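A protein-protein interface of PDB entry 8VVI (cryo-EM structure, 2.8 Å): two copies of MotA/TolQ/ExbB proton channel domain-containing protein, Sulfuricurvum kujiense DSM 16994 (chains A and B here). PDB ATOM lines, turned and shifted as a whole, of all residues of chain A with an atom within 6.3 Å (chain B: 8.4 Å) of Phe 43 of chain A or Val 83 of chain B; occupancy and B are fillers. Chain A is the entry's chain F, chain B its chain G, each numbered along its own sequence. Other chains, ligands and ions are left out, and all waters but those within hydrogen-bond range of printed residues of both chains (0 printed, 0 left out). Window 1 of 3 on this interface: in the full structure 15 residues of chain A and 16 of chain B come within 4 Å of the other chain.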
ATOM      1  N   LEU A  12     -18.700 -12.289  -8.999  1.00  0.00           N
ATOM      2  CA  LEU A  12     -17.551 -12.580  -9.851  1.00  0.00           C
ATOM      3  C   LEU A  12     -16.732 -11.324 -10.126  1.00  0.00           C
ATOM      4  O   LEU A  12     -15.497 -11.373 -10.136  1.00  0.00           O
ATOM      5  CB  LEU A  12     -18.017 -13.214 -11.160  1.00  0.00           C
ATOM      6  CG  LEU A  12     -16.930 -13.826 -12.045  1.00  0.00           C
ATOM      7  CD1 LEU A  12     -16.301 -15.030 -11.365  1.00  0.00           C
ATOM      8  CD2 LEU A  12     -17.497 -14.208 -13.400  1.00  0.00           C
ATOM      9  N   ILE A  38     -15.525  -4.162 -17.094  1.00  0.00           N
ATOM     10  CA  ILE A  38     -16.713  -3.764 -17.842  1.00  0.00           C
ATOM     11  C   ILE A  38     -17.109  -4.848 -18.836  1.00  0.00           C
ATOM     12  O   ILE A  38     -18.298  -5.102 -19.056  1.00  0.00           O
ATOM     13  CB  ILE A  38     -16.482  -2.411 -18.538  1.00  0.00           C
ATOM     14  CG1 ILE A  38     -16.086  -1.344 -17.517  1.00  0.00           C
ATOM     15  CG2 ILE A  38     -17.731  -1.975 -19.284  1.00  0.00           C
ATOM     16  CD1 ILE A  38     -15.548  -0.078 -18.139  1.00  0.00           C
ATOM     17  N   THR A  39     -16.120  -5.505 -19.451  1.00  0.00           N
ATOM     18  CA  THR A  39     -16.417  -6.553 -20.423  1.00  0.00           C
ATOM     19  C   THR A  39     -17.165  -7.712 -19.776  1.00  0.00           C
ATOM     20  O   THR A  39     -18.076  -8.288 -20.382  1.00  0.00           O
ATOM     21  CB  THR A  39     -15.127  -7.047 -21.078  1.00  0.00           C
ATOM     22  OG1 THR A  39     -14.401  -5.930 -21.603  1.00  0.00           O
ATOM     23  CG2 THR A  39     -15.437  -8.013 -22.210  1.00  0.00           C
ATOM     24  N   THR A  40     -16.793  -8.073 -18.546  1.00  0.00           N
ATOM     25  CA  THR A  40     -17.542  -9.099 -17.827  1.00  0.00           C
ATOM     26  C   THR A  40     -18.962  -8.632 -17.537  1.00  0.00           C
ATOM     27  O   THR A  40     -19.903  -9.434 -17.551  1.00  0.00           O
ATOM     28  CB  THR A  40     -16.826  -9.471 -16.531  1.00  0.00           C
ATOM     29  OG1 THR A  40     -15.440  -9.703 -16.802  1.00  0.00           O
ATOM     30  CG2 THR A  40     -17.436 -10.732 -15.943  1.00  0.00           C
ATOM     31  N   GLY A  41     -19.136  -7.338 -17.266  1.00  0.00           N
ATOM     32  CA  GLY A  41     -20.478  -6.796 -17.144  1.00  0.00           C
ATOM     33  C   GLY A  41     -21.266  -6.912 -18.433  1.00  0.00           C
ATOM     34  O   GLY A  41     -22.460  -7.213 -18.416  1.00  0.00           O
ATOM     35  N   ILE A  42     -20.605  -6.676 -19.570  1.00  0.00           N
ATOM     36  CA  ILE A  42     -21.252  -6.868 -20.866  1.00  0.00           C
ATOM     37  C   ILE A  42     -21.623  -8.332 -21.061  1.00  0.00           C
ATOM     38  O   ILE A  42     -22.670  -8.652 -21.639  1.00  0.00           O
ATOM     39  CB  ILE A  42     -20.342  -6.364 -22.002  1.00  0.00           C
ATOM     40  CG1 ILE A  42     -19.947  -4.906 -21.768  1.00  0.00           C
ATOM     41  CG2 ILE A  42     -21.034  -6.509 -23.348  1.00  0.00           C
ATOM     42  CD1 ILE A  42     -19.253  -4.274 -22.948  1.00  0.00           C
ATOM     43  N   PHE A  43     -20.769  -9.242 -20.589  1.00  0.00           N
ATOM     44  CA  PHE A  43     -21.064 -10.666 -20.703  1.00  0.00           C
ATOM     45  C   PHE A  43     -22.326 -11.032 -19.935  1.00  0.00           C
ATOM     46  O   PHE A  43     -23.152 -11.815 -20.418  1.00  0.00           O
ATOM     47  CB  PHE A  43     -19.874 -11.489 -20.206  1.00  0.00           C
ATOM     48  CG  PHE A  43     -20.213 -12.918 -19.895  1.00  0.00           C
ATOM     49  CD1 PHE A  43     -20.580 -13.794 -20.903  1.00  0.00           C
ATOM     50  CD2 PHE A  43     -20.163 -13.387 -18.593  1.00  0.00           C
ATOM     51  CE1 PHE A  43     -20.893 -15.108 -20.616  1.00  0.00           C
ATOM     52  CE2 PHE A  43     -20.476 -14.700 -18.302  1.00  0.00           C
ATOM     53  CZ  PHE A  43     -20.840 -15.561 -19.316  1.00  0.00           C
ATOM     54  N   PHE A  44     -22.499 -10.470 -18.737  1.00  0.00           N
ATOM     55  CA  PHE A  44     -23.671 -10.777 -17.930  1.00  0.00           C
ATOM     56  C   PHE A  44     -24.917 -10.033 -18.390  1.00  0.00           C
ATOM     57  O   PHE A  44     -26.027 -10.431 -18.022  1.00  0.00           O
ATOM     58  CB  PHE A  44     -23.391 -10.471 -16.460  1.00  0.00           C
ATOM     59  CG  PHE A  44     -22.594 -11.538 -15.764  1.00  0.00           C
ATOM     60  CD1 PHE A  44     -23.158 -12.771 -15.487  1.00  0.00           C
ATOM     61  CD2 PHE A  44     -21.280 -11.310 -15.395  1.00  0.00           C
ATOM     62  CE1 PHE A  44     -22.429 -13.756 -14.851  1.00  0.00           C
ATOM     63  CE2 PHE A  44     -20.545 -12.292 -14.759  1.00  0.00           C
ATOM     64  CZ  PHE A  44     -21.120 -13.516 -14.487  1.00  0.00           C
ATOM     65  N   THR A  45     -24.768  -8.965 -19.177  1.00  0.00           N
ATOM     66  CA  THR A  45     -25.934  -8.366 -19.818  1.00  0.00           C
ATOM     67  C   THR A  45     -26.473  -9.278 -20.912  1.00  0.00           C
ATOM     68  O   THR A  45     -27.683  -9.504 -21.004  1.00  0.00           O
ATOM     69  CB  THR A  45     -25.593  -6.990 -20.391  1.00  0.00           C
ATOM     70  OG1 THR A  45     -25.175  -6.115 -19.337  1.00  0.00           O
ATOM     71  CG2 THR A  45     -26.789  -6.393 -21.112  1.00  0.00           C
ATOM     72  N   PHE A  46     -25.582  -9.819 -21.745  1.00  0.00           N
ATOM     73  CA  PHE A  46     -26.004 -10.760 -22.776  1.00  0.00           C
ATOM     74  C   PHE A  46     -26.594 -12.022 -22.158  1.00  0.00           C
ATOM     75  O   PHE A  46     -27.565 -12.581 -22.679  1.00  0.00           O
ATOM     76  CB  PHE A  46     -24.826 -11.106 -23.686  1.00  0.00           C
ATOM     77  CG  PHE A  46     -24.470 -10.015 -24.652  1.00  0.00           C
ATOM     78  CD1 PHE A  46     -25.438  -9.449 -25.463  1.00  0.00           C
ATOM     79  CD2 PHE A  46     -23.170  -9.556 -24.750  1.00  0.00           C
ATOM     80  CE1 PHE A  46     -25.115  -8.446 -26.354  1.00  0.00           C
ATOM     81  CE2 PHE A  46     -22.840  -8.553 -25.640  1.00  0.00           C
ATOM     82  CZ  PHE A  46     -23.814  -7.997 -26.442  1.00  0.00           C
ATOM     83  N   VAL A  47     -26.010 -12.488 -21.053  1.00  0.00           N
ATOM     84  CA  VAL A  47     -26.586 -13.618 -20.329  1.00  0.00           C
ATOM     85  C   VAL A  47     -27.967 -13.255 -19.798  1.00  0.00           C
ATOM     86  O   VAL A  47     -28.895 -14.072 -19.833  1.00  0.00           O
ATOM     87  CB  VAL A  47     -25.638 -14.068 -19.201  1.00  0.00           C
ATOM     88  CG1 VAL A  47     -26.349 -15.009 -18.242  1.00  0.00           C
ATOM     89  CG2 VAL A  47     -24.406 -14.735 -19.784  1.00  0.00           C
ATOM     90  N   GLY A  48     -28.128 -12.022 -19.312  1.00  0.00           N
ATOM     91  CA  GLY A  48     -29.426 -11.596 -18.814  1.00  0.00           C
ATOM     92  C   GLY A  48     -30.508 -11.633 -19.876  1.00  0.00           C
ATOM     93  O   GLY A  48     -31.619 -12.103 -19.625  1.00  0.00           O
ATOM     94  N   ILE B  13     -18.181 -20.014 -32.749  1.00  0.00           N
ATOM     95  CA  ILE B  13     -17.355 -19.217 -31.846  1.00  0.00           C
ATOM     96  C   ILE B  13     -16.473 -20.117 -30.988  1.00  0.00           C
ATOM     97  O   ILE B  13     -15.313 -19.788 -30.712  1.00  0.00           O
ATOM     98  CB  ILE B  13     -18.241 -18.294 -30.990  1.00  0.00           C
ATOM     99  CG1 ILE B  13     -18.909 -17.237 -31.871  1.00  0.00           C
ATOM    100  CG2 ILE B  13     -17.427 -17.620 -29.898  1.00  0.00           C
ATOM    101  CD1 ILE B  13     -20.080 -16.549 -31.215  1.00  0.00           C
ATOM    102  N   PRO B  34      -9.791 -11.508 -29.061  1.00  0.00           N
ATOM    103  CA  PRO B  34     -11.008 -11.030 -28.380  1.00  0.00           C
ATOM    104  C   PRO B  34     -11.888 -10.146 -29.246  1.00  0.00           C
ATOM    105  O   PRO B  34     -13.119 -10.215 -29.142  1.00  0.00           O
ATOM    106  CB  PRO B  34     -10.455 -10.266 -27.167  1.00  0.00           C
ATOM    107  CG  PRO B  34      -9.056  -9.936 -27.521  1.00  0.00           C
ATOM    108  CD  PRO B  34      -8.576 -11.083 -28.343  1.00  0.00           C
ATOM    109  N   ILE B  36     -12.262 -10.241 -32.597  1.00  0.00           N
ATOM    110  CA  ILE B  36     -12.944 -11.055 -33.599  1.00  0.00           C
ATOM    111  C   ILE B  36     -13.992 -11.948 -32.945  1.00  0.00           C
ATOM    112  O   ILE B  36     -15.076 -12.163 -33.500  1.00  0.00           O
ATOM    113  CB  ILE B  36     -11.910 -11.863 -34.402  1.00  0.00           C
ATOM    114  CG1 ILE B  36     -11.007 -10.904 -35.180  1.00  0.00           C
ATOM    115  CG2 ILE B  36     -12.594 -12.839 -35.344  1.00  0.00           C
ATOM    116  CD1 ILE B  36      -9.785 -11.547 -35.762  1.00  0.00           C
ATOM    117  N   LEU B  37     -13.689 -12.484 -31.759  1.00  0.00           N
ATOM    118  CA  LEU B  37     -14.653 -13.330 -31.062  1.00  0.00           C
ATOM    119  C   LEU B  37     -15.910 -12.552 -30.691  1.00  0.00           C
ATOM    120  O   LEU B  37     -17.028 -13.052 -30.856  1.00  0.00           O
ATOM    121  CB  LEU B  37     -14.013 -13.935 -29.812  1.00  0.00           C
ATOM    122  CG  LEU B  37     -13.093 -15.138 -30.023  1.00  0.00           C
ATOM    123  CD1 LEU B  37     -12.134 -15.292 -28.855  1.00  0.00           C
ATOM    124  CD2 LEU B  37     -13.904 -16.405 -30.226  1.00  0.00           C
ATOM    125  N   ILE B  38     -15.748 -11.329 -30.184  1.00  0.00           N
ATOM    126  CA  ILE B  38     -16.908 -10.516 -29.830  1.00  0.00           C
ATOM    127  C   ILE B  38     -17.648 -10.069 -31.083  1.00  0.00           C
ATOM    128  O   ILE B  38     -18.884 -10.083 -31.129  1.00  0.00           O
ATOM    129  CB  ILE B  38     -16.478  -9.318 -28.965  1.00  0.00           C
ATOM    130  CG1 ILE B  38     -15.946  -9.797 -27.617  1.00  0.00           C
ATOM    131  CG2 ILE B  38     -17.644  -8.373 -28.746  1.00  0.00           C
ATOM    132  CD1 ILE B  38     -15.345  -8.697 -26.774  1.00  0.00           C
ATOM    133  N   THR B  39     -16.907  -9.672 -32.121  1.00  0.00           N
ATOM    134  CA  THR B  39     -17.538  -9.215 -33.356  1.00  0.00           C
ATOM    135  C   THR B  39     -18.346 -10.329 -34.010  1.00  0.00           C
ATOM    136  O   THR B  39     -19.432 -10.085 -34.548  1.00  0.00           O
ATOM    137  CB  THR B  39     -16.475  -8.684 -34.318  1.00  0.00           C
ATOM    138  OG1 THR B  39     -15.651  -7.730 -33.638  1.00  0.00           O
ATOM    139  CG2 THR B  39     -17.124  -8.012 -35.514  1.00  0.00           C
ATOM    140  N   THR B  40     -17.828 -11.559 -33.978  1.00  0.00           N
ATOM    141  CA  THR B  40     -18.571 -12.691 -34.522  1.00  0.00           C
ATOM    142  C   THR B  40     -19.864 -12.927 -33.751  1.00  0.00           C
ATOM    143  O   THR B  40     -20.904 -13.228 -34.347  1.00  0.00           O
ATOM    144  CB  THR B  40     -17.701 -13.947 -34.505  1.00  0.00           C
ATOM    145  OG1 THR B  40     -16.371 -13.612 -34.915  1.00  0.00           O
ATOM    146  CG2 THR B  40     -18.266 -15.000 -35.443  1.00  0.00           C
ATOM    147  N   GLY B  41     -19.816 -12.805 -32.423  1.00  0.00           N
ATOM    148  CA  GLY B  41     -21.024 -12.971 -31.631  1.00  0.00           C
ATOM    149  C   GLY B  41     -22.061 -11.903 -31.914  1.00  0.00           C
ATOM    150  O   GLY B  41     -23.257 -12.191 -31.997  1.00  0.00           O
ATOM    151  N   ILE B  42     -21.619 -10.651 -32.057  1.00  0.00           N
ATOM    152  CA  ILE B  42     -22.539  -9.575 -32.409  1.00  0.00           C
ATOM    153  C   ILE B  42     -23.103  -9.785 -33.808  1.00  0.00           C
ATOM    154  O   ILE B  42     -24.267  -9.462 -34.072  1.00  0.00           O
ATOM    155  CB  ILE B  42     -21.840  -8.208 -32.277  1.00  0.00           C
ATOM    156  CG1 ILE B  42     -21.283  -8.026 -30.866  1.00  0.00           C
ATOM    157  CG2 ILE B  42     -22.798  -7.076 -32.613  1.00  0.00           C
ATOM    158  CD1 ILE B  42     -22.336  -8.076 -29.781  1.00  0.00           C
ATOM    159  N   PHE B  76     -29.127 -13.933 -28.682  1.00  0.00           N
ATOM    160  CA  PHE B  76     -28.136 -13.388 -27.765  1.00  0.00           C
ATOM    161  C   PHE B  76     -27.260 -14.455 -27.123  1.00  0.00           C
ATOM    162  O   PHE B  76     -26.394 -14.116 -26.310  1.00  0.00           O
ATOM    163  CB  PHE B  76     -28.828 -12.559 -26.680  1.00  0.00           C
ATOM    164  CG  PHE B  76     -29.845 -11.595 -27.219  1.00  0.00           C
ATOM    165  CD1 PHE B  76     -29.455 -10.360 -27.706  1.00  0.00           C
ATOM    166  CD2 PHE B  76     -31.189 -11.928 -27.246  1.00  0.00           C
ATOM    167  CE1 PHE B  76     -30.387  -9.473 -28.208  1.00  0.00           C
ATOM    168  CE2 PHE B  76     -32.125 -11.044 -27.746  1.00  0.00           C
ATOM    169  CZ  PHE B  76     -31.723  -9.815 -28.226  1.00  0.00           C
ATOM    170  N   TRP B  77     -27.462 -15.730 -27.460  1.00  0.00           N
ATOM    171  CA  TRP B  77     -26.564 -16.767 -26.964  1.00  0.00           C
ATOM    172  C   TRP B  77     -25.203 -16.695 -27.642  1.00  0.00           C
ATOM    173  O   TRP B  77     -24.182 -16.996 -27.014  1.00  0.00           O
ATOM    174  CB  TRP B  77     -27.187 -18.148 -27.166  1.00  0.00           C
ATOM    175  CG  TRP B  77     -28.300 -18.454 -26.211  1.00  0.00           C
ATOM    176  CD1 TRP B  77     -29.611 -18.658 -26.522  1.00  0.00           C
ATOM    177  CD2 TRP B  77     -28.198 -18.599 -24.789  1.00  0.00           C
ATOM    178  NE1 TRP B  77     -30.334 -18.917 -25.384  1.00  0.00           N
ATOM    179  CE2 TRP B  77     -29.489 -18.887 -24.305  1.00  0.00           C
ATOM    180  CE3 TRP B  77     -27.141 -18.512 -23.878  1.00  0.00           C
ATOM    181  CZ2 TRP B  77     -29.753 -19.088 -22.952  1.00  0.00           C
ATOM    182  CZ3 TRP B  77     -27.404 -18.711 -22.535  1.00  0.00           C
ATOM    183  CH2 TRP B  77     -28.699 -18.996 -22.085  1.00  0.00           C
ATOM    184  N   ALA B  78     -25.168 -16.309 -28.919  1.00  0.00           N
ATOM    185  CA  ALA B  78     -23.895 -16.153 -29.613  1.00  0.00           C
ATOM    186  C   ALA B  78     -23.126 -14.946 -29.091  1.00  0.00           C
ATOM    187  O   ALA B  78     -21.896 -14.985 -28.985  1.00  0.00           O
ATOM    188  CB  ALA B  78     -24.127 -16.036 -31.117  1.00  0.00           C
ATOM    189  N   SER B  79     -23.835 -13.859 -28.771  1.00  0.00           N
ATOM    190  CA  SER B  79     -23.177 -12.695 -28.188  1.00  0.00           C
ATOM    191  C   SER B  79     -22.567 -13.030 -26.835  1.00  0.00           C
ATOM    192  O   SER B  79     -21.438 -12.625 -26.537  1.00  0.00           O
ATOM    193  CB  SER B  79     -24.169 -11.542 -28.055  1.00  0.00           C
ATOM    194  OG  SER B  79     -24.292 -10.832 -29.273  1.00  0.00           O
ATOM    195  N   ALA B  80     -23.300 -13.769 -26.000  1.00  0.00           N
ATOM    196  CA  ALA B  80     -22.756 -14.193 -24.715  1.00  0.00           C
ATOM    197  C   ALA B  80     -21.574 -15.135 -24.904  1.00  0.00           C
ATOM    198  O   ALA B  80     -20.589 -15.063 -24.161  1.00  0.00           O
ATOM    199  CB  ALA B  80     -23.847 -14.859 -23.877  1.00  0.00           C
ATOM    200  N   THR B  81     -21.659 -16.030 -25.891  1.00  0.00           N
ATOM    201  CA  THR B  81     -20.555 -16.944 -26.166  1.00  0.00           C
ATOM    202  C   THR B  81     -19.314 -16.192 -26.630  1.00  0.00           C
ATOM    203  O   THR B  81     -18.192 -16.526 -26.234  1.00  0.00           O
ATOM    204  CB  THR B  81     -20.979 -17.973 -27.215  1.00  0.00           C
ATOM    205  OG1 THR B  81     -22.269 -18.497 -26.878  1.00  0.00           O
ATOM    206  CG2 THR B  81     -19.977 -19.113 -27.282  1.00  0.00           C
ATOM    207  N   GLY B  82     -19.494 -15.177 -27.477  1.00  0.00           N
ATOM    208  CA  GLY B  82     -18.350 -14.437 -27.983  1.00  0.00           C
ATOM    209  C   GLY B  82     -17.624 -13.658 -26.903  1.00  0.00           C
ATOM    210  O   GLY B  82     -16.392 -13.660 -26.848  1.00  0.00           O
ATOM    211  N   VAL B  83     -18.375 -12.977 -26.034  1.00  0.00           N
ATOM    212  CA  VAL B  83     -17.755 -12.210 -24.957  1.00  0.00           C
ATOM    213  C   VAL B  83     -17.114 -13.140 -23.935  1.00  0.00           C
ATOM    214  O   VAL B  83     -16.050 -12.836 -23.382  1.00  0.00           O
ATOM    215  CB  VAL B  83     -18.788 -11.273 -24.304  1.00  0.00           C
ATOM    216  CG1 VAL B  83     -18.123 -10.394 -23.260  1.00  0.00           C
ATOM    217  CG2 VAL B  83     -19.467 -10.416 -25.358  1.00  0.00           C
ATOM    218  N   PHE B  84     -17.749 -14.282 -23.661  1.00  0.00           N
ATOM    219  CA  PHE B  84     -17.214 -15.214 -22.674  1.00  0.00           C
ATOM    220  C   PHE B  84     -15.851 -15.746 -23.097  1.00  0.00           C
ATOM    221  O   PHE B  84     -14.910 -15.786 -22.296  1.00  0.00           O
ATOM    222  CB  PHE B  84     -18.195 -16.366 -22.460  1.00  0.00           C
ATOM    223  CG  PHE B  84     -17.653 -17.472 -21.599  1.00  0.00           C
ATOM    224  CD1 PHE B  84     -17.500 -17.295 -20.235  1.00  0.00           C
ATOM    225  CD2 PHE B  84     -17.298 -18.689 -22.156  1.00  0.00           C
ATOM    226  CE1 PHE B  84     -17.002 -18.309 -19.443  1.00  0.00           C
ATOM    227  CE2 PHE B  84     -16.800 -19.707 -21.368  1.00  0.00           C
ATOM    228  CZ  PHE B  84     -16.652 -19.517 -20.010  1.00  0.00           C
ATOM    229  N   PHE B  85     -15.724 -16.160 -24.360  1.00  0.00           N
ATOM    230  CA  PHE B  85     -14.453 -16.697 -24.833  1.00  0.00           C
ATOM    231  C   PHE B  85     -13.427 -15.596 -25.052  1.00  0.00           C
ATOM    232  O   PHE B  85     -12.222 -15.841 -24.924  1.00  0.00           O
ATOM    233  CB  PHE B  85     -14.668 -17.498 -26.114  1.00  0.00           C
ATOM    234  CG  PHE B  85     -15.226 -18.871 -25.878  1.00  0.00           C
ATOM    235  CD1 PHE B  85     -14.617 -19.734 -24.983  1.00  0.00           C
ATOM    236  CD2 PHE B  85     -16.360 -19.297 -26.544  1.00  0.00           C
ATOM    237  CE1 PHE B  85     -15.126 -20.996 -24.762  1.00  0.00           C
ATOM    238  CE2 PHE B  85     -16.874 -20.558 -26.324  1.00  0.00           C
ATOM    239  CZ  PHE B  85     -16.256 -21.409 -25.433  1.00  0.00           C
ATOM    240  N   ALA B  86     -13.877 -14.387 -25.388  1.00  0.00           N
ATOM    241  CA  ALA B  86     -12.961 -13.255 -25.461  1.00  0.00           C
ATOM    242  C   ALA B  86     -12.430 -12.893 -24.081  1.00  0.00           C
ATOM    243  O   ALA B  86     -11.272 -12.481 -23.943  1.00  0.00           O
ATOM    244  CB  ALA B  86     -13.655 -12.056 -26.101  1.00  0.00           C
ATOM    245  N   LEU B  87     -13.266 -13.033 -23.050  1.00  0.00           N
ATOM    246  CA  LEU B  87     -12.811 -12.792 -21.685  1.00  0.00           C
ATOM    247  C   LEU B  87     -11.743 -13.795 -21.276  1.00  0.00           C
ATOM    248  O   LEU B  87     -10.778 -13.440 -20.590  1.00  0.00           O
ATOM    249  CB  LEU B  87     -13.996 -12.850 -20.722  1.00  0.00           C
ATOM    250  CG  LEU B  87     -14.793 -11.560 -20.536  1.00  0.00           C
ATOM    251  CD1 LEU B  87     -16.109 -11.851 -19.836  1.00  0.00           C
ATOM    252  CD2 LEU B  87     -13.980 -10.538 -19.760  1.00  0.00           C
ATOM    253  N   ILE B  88     -11.900 -15.056 -21.685  1.00  0.00           N
ATOM    254  CA  ILE B  88     -10.907 -16.078 -21.363  1.00  0.00           C
ATOM    255  C   ILE B  88      -9.564 -15.732 -21.989  1.00  0.00           C
ATOM    256  O   ILE B  88      -8.511 -15.866 -21.352  1.00  0.00           O
ATOM    257  CB  ILE B  88     -11.404 -17.464 -21.814  1.00  0.00           C
ATOM    258  CG1 ILE B  88     -12.677 -17.845 -21.057  1.00  0.00           C
ATOM    259  CG2 ILE B  88     -10.326 -18.515 -21.607  1.00  0.00           C
ATOM    260  CD1 ILE B  88     -13.202 -19.218 -21.405  1.00  0.00           C
ATOM    261  N   ILE B  89      -9.574 -15.280 -23.244  1.00  0.00           N
ATOM    262  CA  ILE B  89      -8.336 -14.865 -23.896  1.00  0.00           C
ATOM    263  C   ILE B  89      -7.725 -13.675 -23.167  1.00  0.00           C
ATOM    264  O   ILE B  89      -6.510 -13.623 -22.938  1.00  0.00           O
ATOM    265  CB  ILE B  89      -8.592 -14.551 -25.381  1.00  0.00           C
ATOM    266  CG1 ILE B  89      -9.074 -15.804 -26.117  1.00  0.00           C
ATOM    267  CG2 ILE B  89      -7.338 -14.000 -26.039  1.00  0.00           C
ATOM    268  CD1 ILE B  89      -8.064 -16.930 -26.136  1.00  0.00           C
ATOM    269  N   LYS B  90      -8.556 -12.699 -22.792  1.00  0.00           N
ATOM    270  CA  LYS B  90      -8.061 -11.548 -22.044  1.00  0.00           C
ATOM    271  C   LYS B  90      -7.572 -11.952 -20.658  1.00  0.00           C
ATOM    272  O   LYS B  90      -6.550 -11.444 -20.183  1.00  0.00           O
ATOM    273  CB  LYS B  90      -9.151 -10.483 -21.941  1.00  0.00           C
ATOM    274  CG  LYS B  90      -9.527  -9.850 -23.269  1.00  0.00           C
ATOM    275  CD  LYS B  90     -10.118  -8.466 -23.073  1.00  0.00           C
ATOM    276  CE  LYS B  90     -11.633  -8.497 -23.165  1.00  0.00           C
ATOM    277  NZ  LYS B  90     -12.100  -8.629 -24.573  1.00  0.00           N
ATOM    278  N   ILE B  91      -8.294 -12.854 -19.990  1.00  0.00           N
ATOM    279  CA  ILE B  91      -7.868 -13.327 -18.676  1.00  0.00           C
ATOM    280  C   ILE B  91      -6.553 -14.090 -18.784  1.00  0.00           C
ATOM    281  O   ILE B  91      -5.662 -13.941 -17.940  1.00  0.00           O
ATOM    282  CB  ILE B  91      -8.975 -14.181 -18.030  1.00  0.00           C
ATOM    283  CG1 ILE B  91     -10.052 -13.281 -17.421  1.00  0.00           C
ATOM    284  CG2 ILE B  91      -8.399 -15.112 -16.975  1.00  0.00           C
ATOM    285  CD1 ILE B  91     -11.333 -14.008 -17.086  1.00  0.00           C
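Phe 43 of chain A touches four residues of chain B. No residue of chain B comes within 4 Å of Gly 41 of chain A. No residue of chain B comes within 4 Å of Phe 44 of chain A. Of the printed residues of chain A, Ala 80 of chain B touches Phe 43 and Phe 46. Of the printed residues of chain A, Leu 87 of chain B touches Thr 39 (3.8 Å), Thr 40 (3.4 Å) and Phe 43 (3.8 Å). Ile 42 of chain A touches none of the printed residues of chain B. Ile 91 of chain B touches none of the printed residues of chain A. The nearest residue of chain A that does not touch Val 83 of chain B is Ile 42 of chain A (4.6 Å). The nearest printed residue of chain A that does not touch Ser 79 of chain B is Phe 43 of chain A (5.8 Å).
The side-chain hydroxyl of Ser 79 of chain B is in hydrogen-bond range of the backbone carbonyl oxygen of Gly 41 of chain B (3.2 Å).
Positions printed for both chains: 38, 39, 40, 41 and 42.
Printed residues of chain A that touch a printed residue of chain B: Thr 39, Thr 40, Phe 43 and Phe 46. Hydrophobic or aromatic side chains of chain A that line the printed part of chain B: Phe 43 and Phe 46. Among the printed residues, no Asp or Glu carboxylate lies within 4 Å of a Lys or Arg side-chain nitrogen of the other chain.
Among the printed residues, pairs that only touch across the chains: Thr 39 of chain A with Val 83 of chain B (3.6 Å), Thr 39 of chain A with Leu 87 of chain B (3.8 Å), Thr 39 of chain A with Lys 90 of chain B (3.95 Å), Thr 40 of chain A with Leu 87 of chain B (3.4 Å), Phe 43 of chain A with Ala 80 of chain B (3.5 Å), Phe 43 of chain A with Val 83 of chain B (3.7 Å), Phe 43 of chain A with Phe 84 of chain B (3.5 Å), Phe 43 of chain A with Leu 87 of chain B (3.8 Å), Phe 46 of chain A with Ile 42 of chain B (3.7 Å), Phe 46 of chain A with Ser 79 of chain B (3.6 Å), Phe 46 of chain A with Ala 80 of chain B (3.8 Å) and Phe 46 of chain A with Val 83 of chain B (3.8 Å).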
